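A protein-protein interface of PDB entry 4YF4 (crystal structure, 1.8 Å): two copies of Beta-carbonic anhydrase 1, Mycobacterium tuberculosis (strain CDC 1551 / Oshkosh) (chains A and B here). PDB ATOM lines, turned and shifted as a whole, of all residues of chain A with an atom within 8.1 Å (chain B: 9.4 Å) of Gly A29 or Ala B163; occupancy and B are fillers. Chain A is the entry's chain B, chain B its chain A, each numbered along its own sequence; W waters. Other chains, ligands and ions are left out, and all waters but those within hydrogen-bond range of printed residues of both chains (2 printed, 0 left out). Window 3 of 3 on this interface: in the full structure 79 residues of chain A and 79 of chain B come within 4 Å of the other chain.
O of Leu A31 is in hydrogen-bond range of NH1 of Arg B48 (3.1 Å).
The side-chain carboxylate (OD2) of Asp B99 is in salt-bridge range of the guanidinium group (NH1) of Arg B48, 2.8 Å away. OG1 of Thr B98 is in hydrogen-bond range of N of Val B162. OD1 of Asp B161 is in hydrogen-bond range of N of Ala B163, at 2.8 Å. N of Thr B164 sits at hydrogen-bond distance from OD1 of Asp B161 (3.2 Å). The backbone NH (N) of Asp B161 sits at hydrogen-bond distance from the backbone carbonyl oxygen (O) of Lys B166 (3.0 Å). The side-chain hydroxyl (OG1) of Thr B164 sits close to the backbone NH (N) of Lys B166.
Among the printed residues, pairs that only touch across the chains: Pro A30 with Val B162 (3.2 Å), Phe A27 with Val B162 (3.3 Å), Pro A32 with Arg B48 (3.4 Å), Phe A27 with Thr B164 (3.5 Å), Phe A27 with Gly B165 (3.5 Å), Ala A24 with Thr B164 (3.6 Å), Gly A29 with Ala B163 (3.7 Å), Ala A24 with Lys B166 (3.7 Å), Phe A27 with Ala B163 (3.8 Å), Pro A30 with Ala B163 (3.8 Å) and Ala A24 with Gly B165 (3.9 Å).
Gly A29 touches just one residue of chain B: Ala B163 (3.7 Å). Printed residues of chain A within 4 Å of Val B162: Phe A27 (3.3 Å) and Pro A30 (3.2 Å). Printed residues of chain A within 4 Å of Lys B166: Ala A24 (3.7 Å). Of the printed residues of chain A, Gly B165 touches Ala A24 and Phe A27. Of the printed residues of chain A, Thr B164 touches Ala A24 and Phe A27. Asp B161 touches none of the printed residues of chain A. Thr B98 touches none of the printed residues of chain A. The nearest printed residue of chain B that does not touch Phe A27 is Phe B160 (4.2 Å).
Of the 15 printed residues of chain B, 6 touch a printed residue of chain A. Printed residues of chain A that touch a printed residue of chain B: Ala A24, Phe A27, Gly A29, Pro A30, Leu A31 and Pro A32. Hydrophobic or aromatic side chains of chain A that line the printed part of chain B: Ala A24, Phe A27, Pro A30 and Leu A31. Among the printed residues, 12 pairs touch across the chains. Among the printed residues, no Asp or Glu carboxylate lies within 4 Å of a Lys or Arg side-chain nitrogen of the other chain.
No position is printed for both chains. Of the 12 pairs that touch across the chains among the printed residues, none has its exchanged pair printed and touching as well.
Water W1 bridges the backbone carbonyl oxygen of Val B162 (2.7 Å) and the backbone NH of Leu A31 (2.9 Å). Water W2 bridges O of Arg B48 (3.0 Å) and OE2 of Glu A59 (3.2 Å).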
ATOM      1  N   ALA A  24      -3.287  18.669  19.887  1.00  0.00           N
ATOM      2  CA  ALA A  24      -3.446  17.921  18.643  1.00  0.00           C
ATOM      3  C   ALA A  24      -2.258  17.007  18.386  1.00  0.00           C
ATOM      4  O   ALA A  24      -2.413  15.946  17.782  1.00  0.00           O
ATOM      5  CB  ALA A  24      -3.630  18.872  17.478  1.00  0.00           C
ATOM      6  N   GLY A  26      -0.584  15.251  20.492  1.00  0.00           N
ATOM      7  CA  GLY A  26      -0.687  14.017  21.255  1.00  0.00           C
ATOM      8  C   GLY A  26      -2.018  13.300  21.115  1.00  0.00           C
ATOM      9  O   GLY A  26      -2.291  12.333  21.829  1.00  0.00           O
ATOM     10  N   PHE A  27      -2.845  13.760  20.184  1.00  0.00           N
ATOM     11  CA  PHE A  27      -4.188  13.218  20.017  1.00  0.00           C
ATOM     12  C   PHE A  27      -4.211  11.814  19.425  1.00  0.00           C
ATOM     13  O   PHE A  27      -3.409  11.472  18.548  1.00  0.00           O
ATOM     14  CB  PHE A  27      -5.022  14.146  19.135  1.00  0.00           C
ATOM     15  CG  PHE A  27      -6.472  13.759  19.038  1.00  0.00           C
ATOM     16  CD1 PHE A  27      -7.330  13.973  20.107  1.00  0.00           C
ATOM     17  CD2 PHE A  27      -6.979  13.197  17.876  1.00  0.00           C
ATOM     18  CE1 PHE A  27      -8.665  13.629  20.025  1.00  0.00           C
ATOM     19  CE2 PHE A  27      -8.314  12.850  17.779  1.00  0.00           C
ATOM     20  CZ  PHE A  27      -9.166  13.074  18.860  1.00  0.00           C
ATOM     21  N   LYS A  28      -5.150  11.006  19.903  1.00  0.00           N
ATOM     22  CA  LYS A  28      -5.405   9.696  19.310  1.00  0.00           C
ATOM     23  C   LYS A  28      -6.882   9.568  18.943  1.00  0.00           C
ATOM     24  O   LYS A  28      -7.763   9.726  19.796  1.00  0.00           O
ATOM     25  CB  LYS A  28      -4.986   8.577  20.264  1.00  0.00           C
ATOM     26  CG  LYS A  28      -3.509   8.580  20.580  1.00  0.00           C
ATOM     27  CD  LYS A  28      -3.139   7.487  21.573  1.00  0.00           C
ATOM     28  CE  LYS A  28      -3.281   6.105  20.963  1.00  0.00           C
ATOM     29  NZ  LYS A  28      -2.766   5.048  21.881  1.00  0.00           N
ATOM     30  N   GLY A  29      -7.149   9.300  17.668  1.00  0.00           N
ATOM     31  CA  GLY A  29      -8.515   9.217  17.180  1.00  0.00           C
ATOM     32  C   GLY A  29      -8.533   8.792  15.729  1.00  0.00           C
ATOM     33  O   GLY A  29      -7.475   8.554  15.148  1.00  0.00           O
ATOM     34  N   PRO A  30      -9.729   8.712  15.124  1.00  0.00           N
ATOM     35  CA  PRO A  30     -11.012   9.078  15.732  1.00  0.00           C
ATOM     36  C   PRO A  30     -11.636   7.933  16.526  1.00  0.00           C
ATOM     37  O   PRO A  30     -11.379   6.768  16.223  1.00  0.00           O
ATOM     38  CB  PRO A  30     -11.877   9.376  14.510  1.00  0.00           C
ATOM     39  CG  PRO A  30     -11.378   8.401  13.489  1.00  0.00           C
ATOM     40  CD  PRO A  30      -9.887   8.312  13.714  1.00  0.00           C
ATOM     41  N   LEU A  31     -12.449   8.269  17.522  1.00  0.00           N
ATOM     42  CA  LEU A  31     -13.164   7.276  18.313  1.00  0.00           C
ATOM     43  C   LEU A  31     -14.596   7.171  17.799  1.00  0.00           C
ATOM     44  O   LEU A  31     -15.048   8.040  17.062  1.00  0.00           O
ATOM     45  CB  LEU A  31     -13.175   7.679  19.787  1.00  0.00           C
ATOM     46  CG  LEU A  31     -11.828   7.933  20.462  1.00  0.00           C
ATOM     47  CD1 LEU A  31     -12.048   8.200  21.944  1.00  0.00           C
ATOM     48  CD2 LEU A  31     -10.888   6.761  20.250  1.00  0.00           C
ATOM     49  N   PRO A  32     -15.315   6.099  18.173  1.00  0.00           N
ATOM     50  CA  PRO A  32     -16.729   5.987  17.783  1.00  0.00           C
ATOM     51  C   PRO A  32     -17.599   7.081  18.409  1.00  0.00           C
ATOM     52  O   PRO A  32     -17.282   7.609  19.480  1.00  0.00           O
ATOM     53  CB  PRO A  32     -17.136   4.618  18.337  1.00  0.00           C
ATOM     54  CG  PRO A  32     -15.863   3.865  18.475  1.00  0.00           C
ATOM     55  CD  PRO A  32     -14.830   4.877  18.836  1.00  0.00           C
ATOM     56  N   GLU A  59     -11.778  10.433  27.184  1.00  0.00           N
ATOM     57  CA  GLU A  59     -12.382  10.770  25.901  1.00  0.00           C
ATOM     58  C   GLU A  59     -13.197   9.576  25.381  1.00  0.00           C
ATOM     59  O   GLU A  59     -12.794   8.430  25.545  1.00  0.00           O
ATOM     60  CB  GLU A  59     -11.302  11.204  24.895  1.00  0.00           C
ATOM     61  CG  GLU A  59     -10.671  12.570  25.216  1.00  0.00           C
ATOM     62  CD  GLU A  59      -9.572  12.977  24.239  1.00  0.00           C
ATOM     63  OE1 GLU A  59      -8.745  13.847  24.601  1.00  0.00           O
ATOM     64  OE2 GLU A  59      -9.535  12.441  23.112  1.00  0.00           O
ATOM     65  N   ARG B  48     -16.492  12.741  22.433  1.00  0.00           N
ATOM     66  CA  ARG B  48     -15.114  12.793  21.956  1.00  0.00           C
ATOM     67  C   ARG B  48     -14.485  14.168  22.169  1.00  0.00           C
ATOM     68  O   ARG B  48     -13.341  14.396  21.795  1.00  0.00           O
ATOM     69  CB  ARG B  48     -15.036  12.363  20.488  1.00  0.00           C
ATOM     70  CG  ARG B  48     -15.407  10.891  20.271  1.00  0.00           C
ATOM     71  CD  ARG B  48     -15.714  10.590  18.806  1.00  0.00           C
ATOM     72  NE  ARG B  48     -16.871  11.346  18.335  1.00  0.00           N
ATOM     73  CZ  ARG B  48     -17.421  11.213  17.130  1.00  0.00           C
ATOM     74  NH1 ARG B  48     -16.937  10.330  16.259  1.00  0.00           N
ATOM     75  NH2 ARG B  48     -18.466  11.957  16.806  1.00  0.00           N
ATOM     76  N   LEU B  49     -15.236  15.079  22.782  1.00  0.00           N
ATOM     77  CA  LEU B  49     -14.742  16.435  23.007  1.00  0.00           C
ATOM     78  C   LEU B  49     -14.438  16.703  24.468  1.00  0.00           C
ATOM     79  O   LEU B  49     -15.336  16.987  25.255  1.00  0.00           O
ATOM     80  CB  LEU B  49     -15.728  17.494  22.486  1.00  0.00           C
ATOM     81  CG  LEU B  49     -15.595  17.863  21.008  1.00  0.00           C
ATOM     82  CD1 LEU B  49     -15.802  16.650  20.094  1.00  0.00           C
ATOM     83  CD2 LEU B  49     -16.590  18.956  20.668  1.00  0.00           C
ATOM     84  N   HIS B  97     -18.022  20.212  15.386  1.00  0.00           N
ATOM     85  CA  HIS B  97     -17.002  19.214  15.093  1.00  0.00           C
ATOM     86  C   HIS B  97     -17.404  18.281  13.956  1.00  0.00           C
ATOM     87  O   HIS B  97     -18.574  18.244  13.565  1.00  0.00           O
ATOM     88  CB  HIS B  97     -16.703  18.398  16.346  1.00  0.00           C
ATOM     89  CG  HIS B  97     -17.822  17.508  16.753  1.00  0.00           C
ATOM     90  ND1 HIS B  97     -17.939  16.211  16.303  1.00  0.00           N
ATOM     91  CD2 HIS B  97     -18.886  17.726  17.556  1.00  0.00           C
ATOM     92  CE1 HIS B  97     -19.018  15.664  16.826  1.00  0.00           C
ATOM     93  NE2 HIS B  97     -19.610  16.563  17.589  1.00  0.00           N
ATOM     94  N   THR B  98     -16.435  17.520  13.443  1.00  0.00           N
ATOM     95  CA  THR B  98     -16.720  16.528  12.398  1.00  0.00           C
ATOM     96  C   THR B  98     -17.385  15.276  12.996  1.00  0.00           C
ATOM     97  O   THR B  98     -17.263  15.014  14.197  1.00  0.00           O
ATOM     98  CB  THR B  98     -15.458  16.136  11.594  1.00  0.00           C
ATOM     99  OG1 THR B  98     -14.488  15.533  12.463  1.00  0.00           O
ATOM    100  CG2 THR B  98     -14.847  17.365  10.915  1.00  0.00           C
ATOM    101  N   ASP B  99     -18.086  14.517  12.154  1.00  0.00           N
ATOM    102  CA  ASP B  99     -18.843  13.331  12.588  1.00  0.00           C
ATOM    103  C   ASP B  99     -19.808  13.625  13.736  1.00  0.00           C
ATOM    104  O   ASP B  99     -19.883  12.866  14.704  1.00  0.00           O
ATOM    105  CB  ASP B  99     -17.894  12.197  12.990  1.00  0.00           C
ATOM    106  CG  ASP B  99     -18.566  10.827  12.956  1.00  0.00           C
ATOM    107  OD1 ASP B  99     -19.308  10.544  11.997  1.00  0.00           O
ATOM    108  OD2 ASP B  99     -18.360  10.038  13.895  1.00  0.00           O
ATOM    109  N   VAL B 159     -14.495  24.288  13.804  1.00  0.00           N
ATOM    110  CA  VAL B 159     -14.891  22.894  13.707  1.00  0.00           C
ATOM    111  C   VAL B 159     -13.734  22.040  14.217  1.00  0.00           C
ATOM    112  O   VAL B 159     -12.617  22.148  13.720  1.00  0.00           O
ATOM    113  CB  VAL B 159     -15.213  22.480  12.246  1.00  0.00           C
ATOM    114  CG1 VAL B 159     -15.557  20.982  12.174  1.00  0.00           C
ATOM    115  CG2 VAL B 159     -16.328  23.335  11.675  1.00  0.00           C
ATOM    116  N   PHE B 160     -13.999  21.214  15.225  1.00  0.00           N
ATOM    117  CA  PHE B 160     -13.004  20.302  15.793  1.00  0.00           C
ATOM    118  C   PHE B 160     -12.979  19.012  14.974  1.00  0.00           C
ATOM    119  O   PHE B 160     -14.016  18.370  14.799  1.00  0.00           O
ATOM    120  CB  PHE B 160     -13.400  19.972  17.238  1.00  0.00           C
ATOM    121  CG  PHE B 160     -12.497  18.962  17.925  1.00  0.00           C
ATOM    122  CD1 PHE B 160     -11.177  19.272  18.241  1.00  0.00           C
ATOM    123  CD2 PHE B 160     -12.997  17.723  18.310  1.00  0.00           C
ATOM    124  CE1 PHE B 160     -10.353  18.336  18.898  1.00  0.00           C
ATOM    125  CE2 PHE B 160     -12.196  16.795  18.978  1.00  0.00           C
ATOM    126  CZ  PHE B 160     -10.870  17.093  19.269  1.00  0.00           C
ATOM    127  N   ASP B 161     -11.806  18.634  14.477  1.00  0.00           N
ATOM    128  CA  ASP B 161     -11.662  17.403  13.699  1.00  0.00           C
ATOM    129  C   ASP B 161     -11.446  16.235  14.666  1.00  0.00           C
ATOM    130  O   ASP B 161     -10.382  16.109  15.265  1.00  0.00           O
ATOM    131  CB  ASP B 161     -10.494  17.544  12.693  1.00  0.00           C
ATOM    132  CG  ASP B 161     -10.340  16.332  11.764  1.00  0.00           C
ATOM    133  OD1 ASP B 161     -10.619  15.193  12.184  1.00  0.00           O
ATOM    134  OD2 ASP B 161      -9.914  16.514  10.593  1.00  0.00           O
ATOM    135  N   VAL B 162     -12.451  15.372  14.808  1.00  0.00           N
ATOM    136  CA  VAL B 162     -12.369  14.288  15.794  1.00  0.00           C
ATOM    137  C   VAL B 162     -11.341  13.215  15.441  1.00  0.00           C
ATOM    138  O   VAL B 162     -11.118  12.284  16.214  1.00  0.00           O
ATOM    139  CB  VAL B 162     -13.721  13.596  16.004  1.00  0.00           C
ATOM    140  CG1 VAL B 162     -14.745  14.579  16.539  1.00  0.00           C
ATOM    141  CG2 VAL B 162     -14.185  12.938  14.706  1.00  0.00           C
ATOM    142  N   ALA B 163     -10.734  13.334  14.264  1.00  0.00           N
ATOM    143  CA  ALA B 163      -9.728  12.382  13.821  1.00  0.00           C
ATOM    144  C   ALA B 163      -8.311  12.924  14.028  1.00  0.00           C
ATOM    145  O   ALA B 163      -7.365  12.157  14.169  1.00  0.00           O
ATOM    146  CB  ALA B 163      -9.949  12.014  12.353  1.00  0.00           C
ATOM    147  N   THR B 164      -8.174  14.244  14.068  1.00  0.00           N
ATOM    148  CA  THR B 164      -6.846  14.860  14.171  1.00  0.00           C
ATOM    149  C   THR B 164      -6.647  15.673  15.454  1.00  0.00           C
ATOM    150  O   THR B 164      -5.516  15.925  15.868  1.00  0.00           O
ATOM    151  CB  THR B 164      -6.585  15.794  12.987  1.00  0.00           C
ATOM    152  OG1 THR B 164      -7.442  16.939  13.083  1.00  0.00           O
ATOM    153  CG2 THR B 164      -6.850  15.074  11.665  1.00  0.00           C
ATOM    154  N   GLY B 165      -7.749  16.113  16.051  1.00  0.00           N
ATOM    155  CA  GLY B 165      -7.713  16.914  17.266  1.00  0.00           C
ATOM    156  C   GLY B 165      -7.503  18.400  17.037  1.00  0.00           C
ATOM    157  O   GLY B 165      -7.457  19.185  17.988  1.00  0.00           O
ATOM    158  N   LYS B 166      -7.368  18.783  15.769  1.00  0.00           N
ATOM    159  CA  LYS B 166      -7.138  20.175  15.396  1.00  0.00           C
ATOM    160  C   LYS B 166      -8.446  20.966  15.302  1.00  0.00           C
ATOM    161  O   LYS B 166      -9.514  20.414  15.045  1.00  0.00           O
ATOM    162  CB  LYS B 166      -6.378  20.257  14.060  1.00  0.00           C
ATOM    163  CG  LYS B 166      -5.002  19.625  14.084  1.00  0.00           C
ATOM    164  CD  LYS B 166      -4.333  19.650  12.704  1.00  0.00           C
ATOM    165  CE  LYS B 166      -2.984  18.947  12.749  1.00  0.00           C
ATOM    166  NZ  LYS B 166      -2.330  18.889  11.407  1.00  0.00           N
ATOM    167  N   LEU B 167      -8.344  22.269  15.521  1.00  0.00           N
ATOM    168  CA  LEU B 167      -9.467  23.169  15.336  1.00  0.00           C
ATOM    169  C   LEU B 167      -9.302  23.961  14.037  1.00  0.00           C
ATOM    170  O   LEU B 167      -8.223  24.473  13.737  1.00  0.00           O
ATOM    171  CB  LEU B 167      -9.578  24.116  16.528  1.00  0.00           C
ATOM    172  CG  LEU B 167     -10.045  23.462  17.816  1.00  0.00           C
ATOM    173  CD1 LEU B 167      -9.741  24.379  18.989  1.00  0.00           C
ATOM    174  CD2 LEU B 167     -11.537  23.163  17.710  1.00  0.00           C
ATOM    175  N   ASN B 168     -10.374  24.045  13.259  1.00  0.00           N
ATOM    176  CA  ASN B 168     -10.342  24.786  12.009  1.00  0.00           C
ATOM    177  C   ASN B 168     -11.357  25.922  12.030  1.00  0.00           C
ATOM    178  O   ASN B 168     -12.551  25.690  12.165  1.00  0.00           O
ATOM    179  CB  ASN B 168     -10.598  23.832  10.850  1.00  0.00           C
ATOM    180  CG  ASN B 168      -9.437  22.889  10.628  1.00  0.00           C
ATOM    181  OD1 ASN B 168      -8.292  23.322  10.544  1.00  0.00           O
ATOM    182  ND2 ASN B 168      -9.719  21.591  10.562  1.00  0.00           N
HETATM  183  O   HOH W   1     -12.080  11.012  18.427  1.00  0.00           O
HETATM  184  O   HOH W   2     -11.804  12.013  20.935  1.00  0.00           O
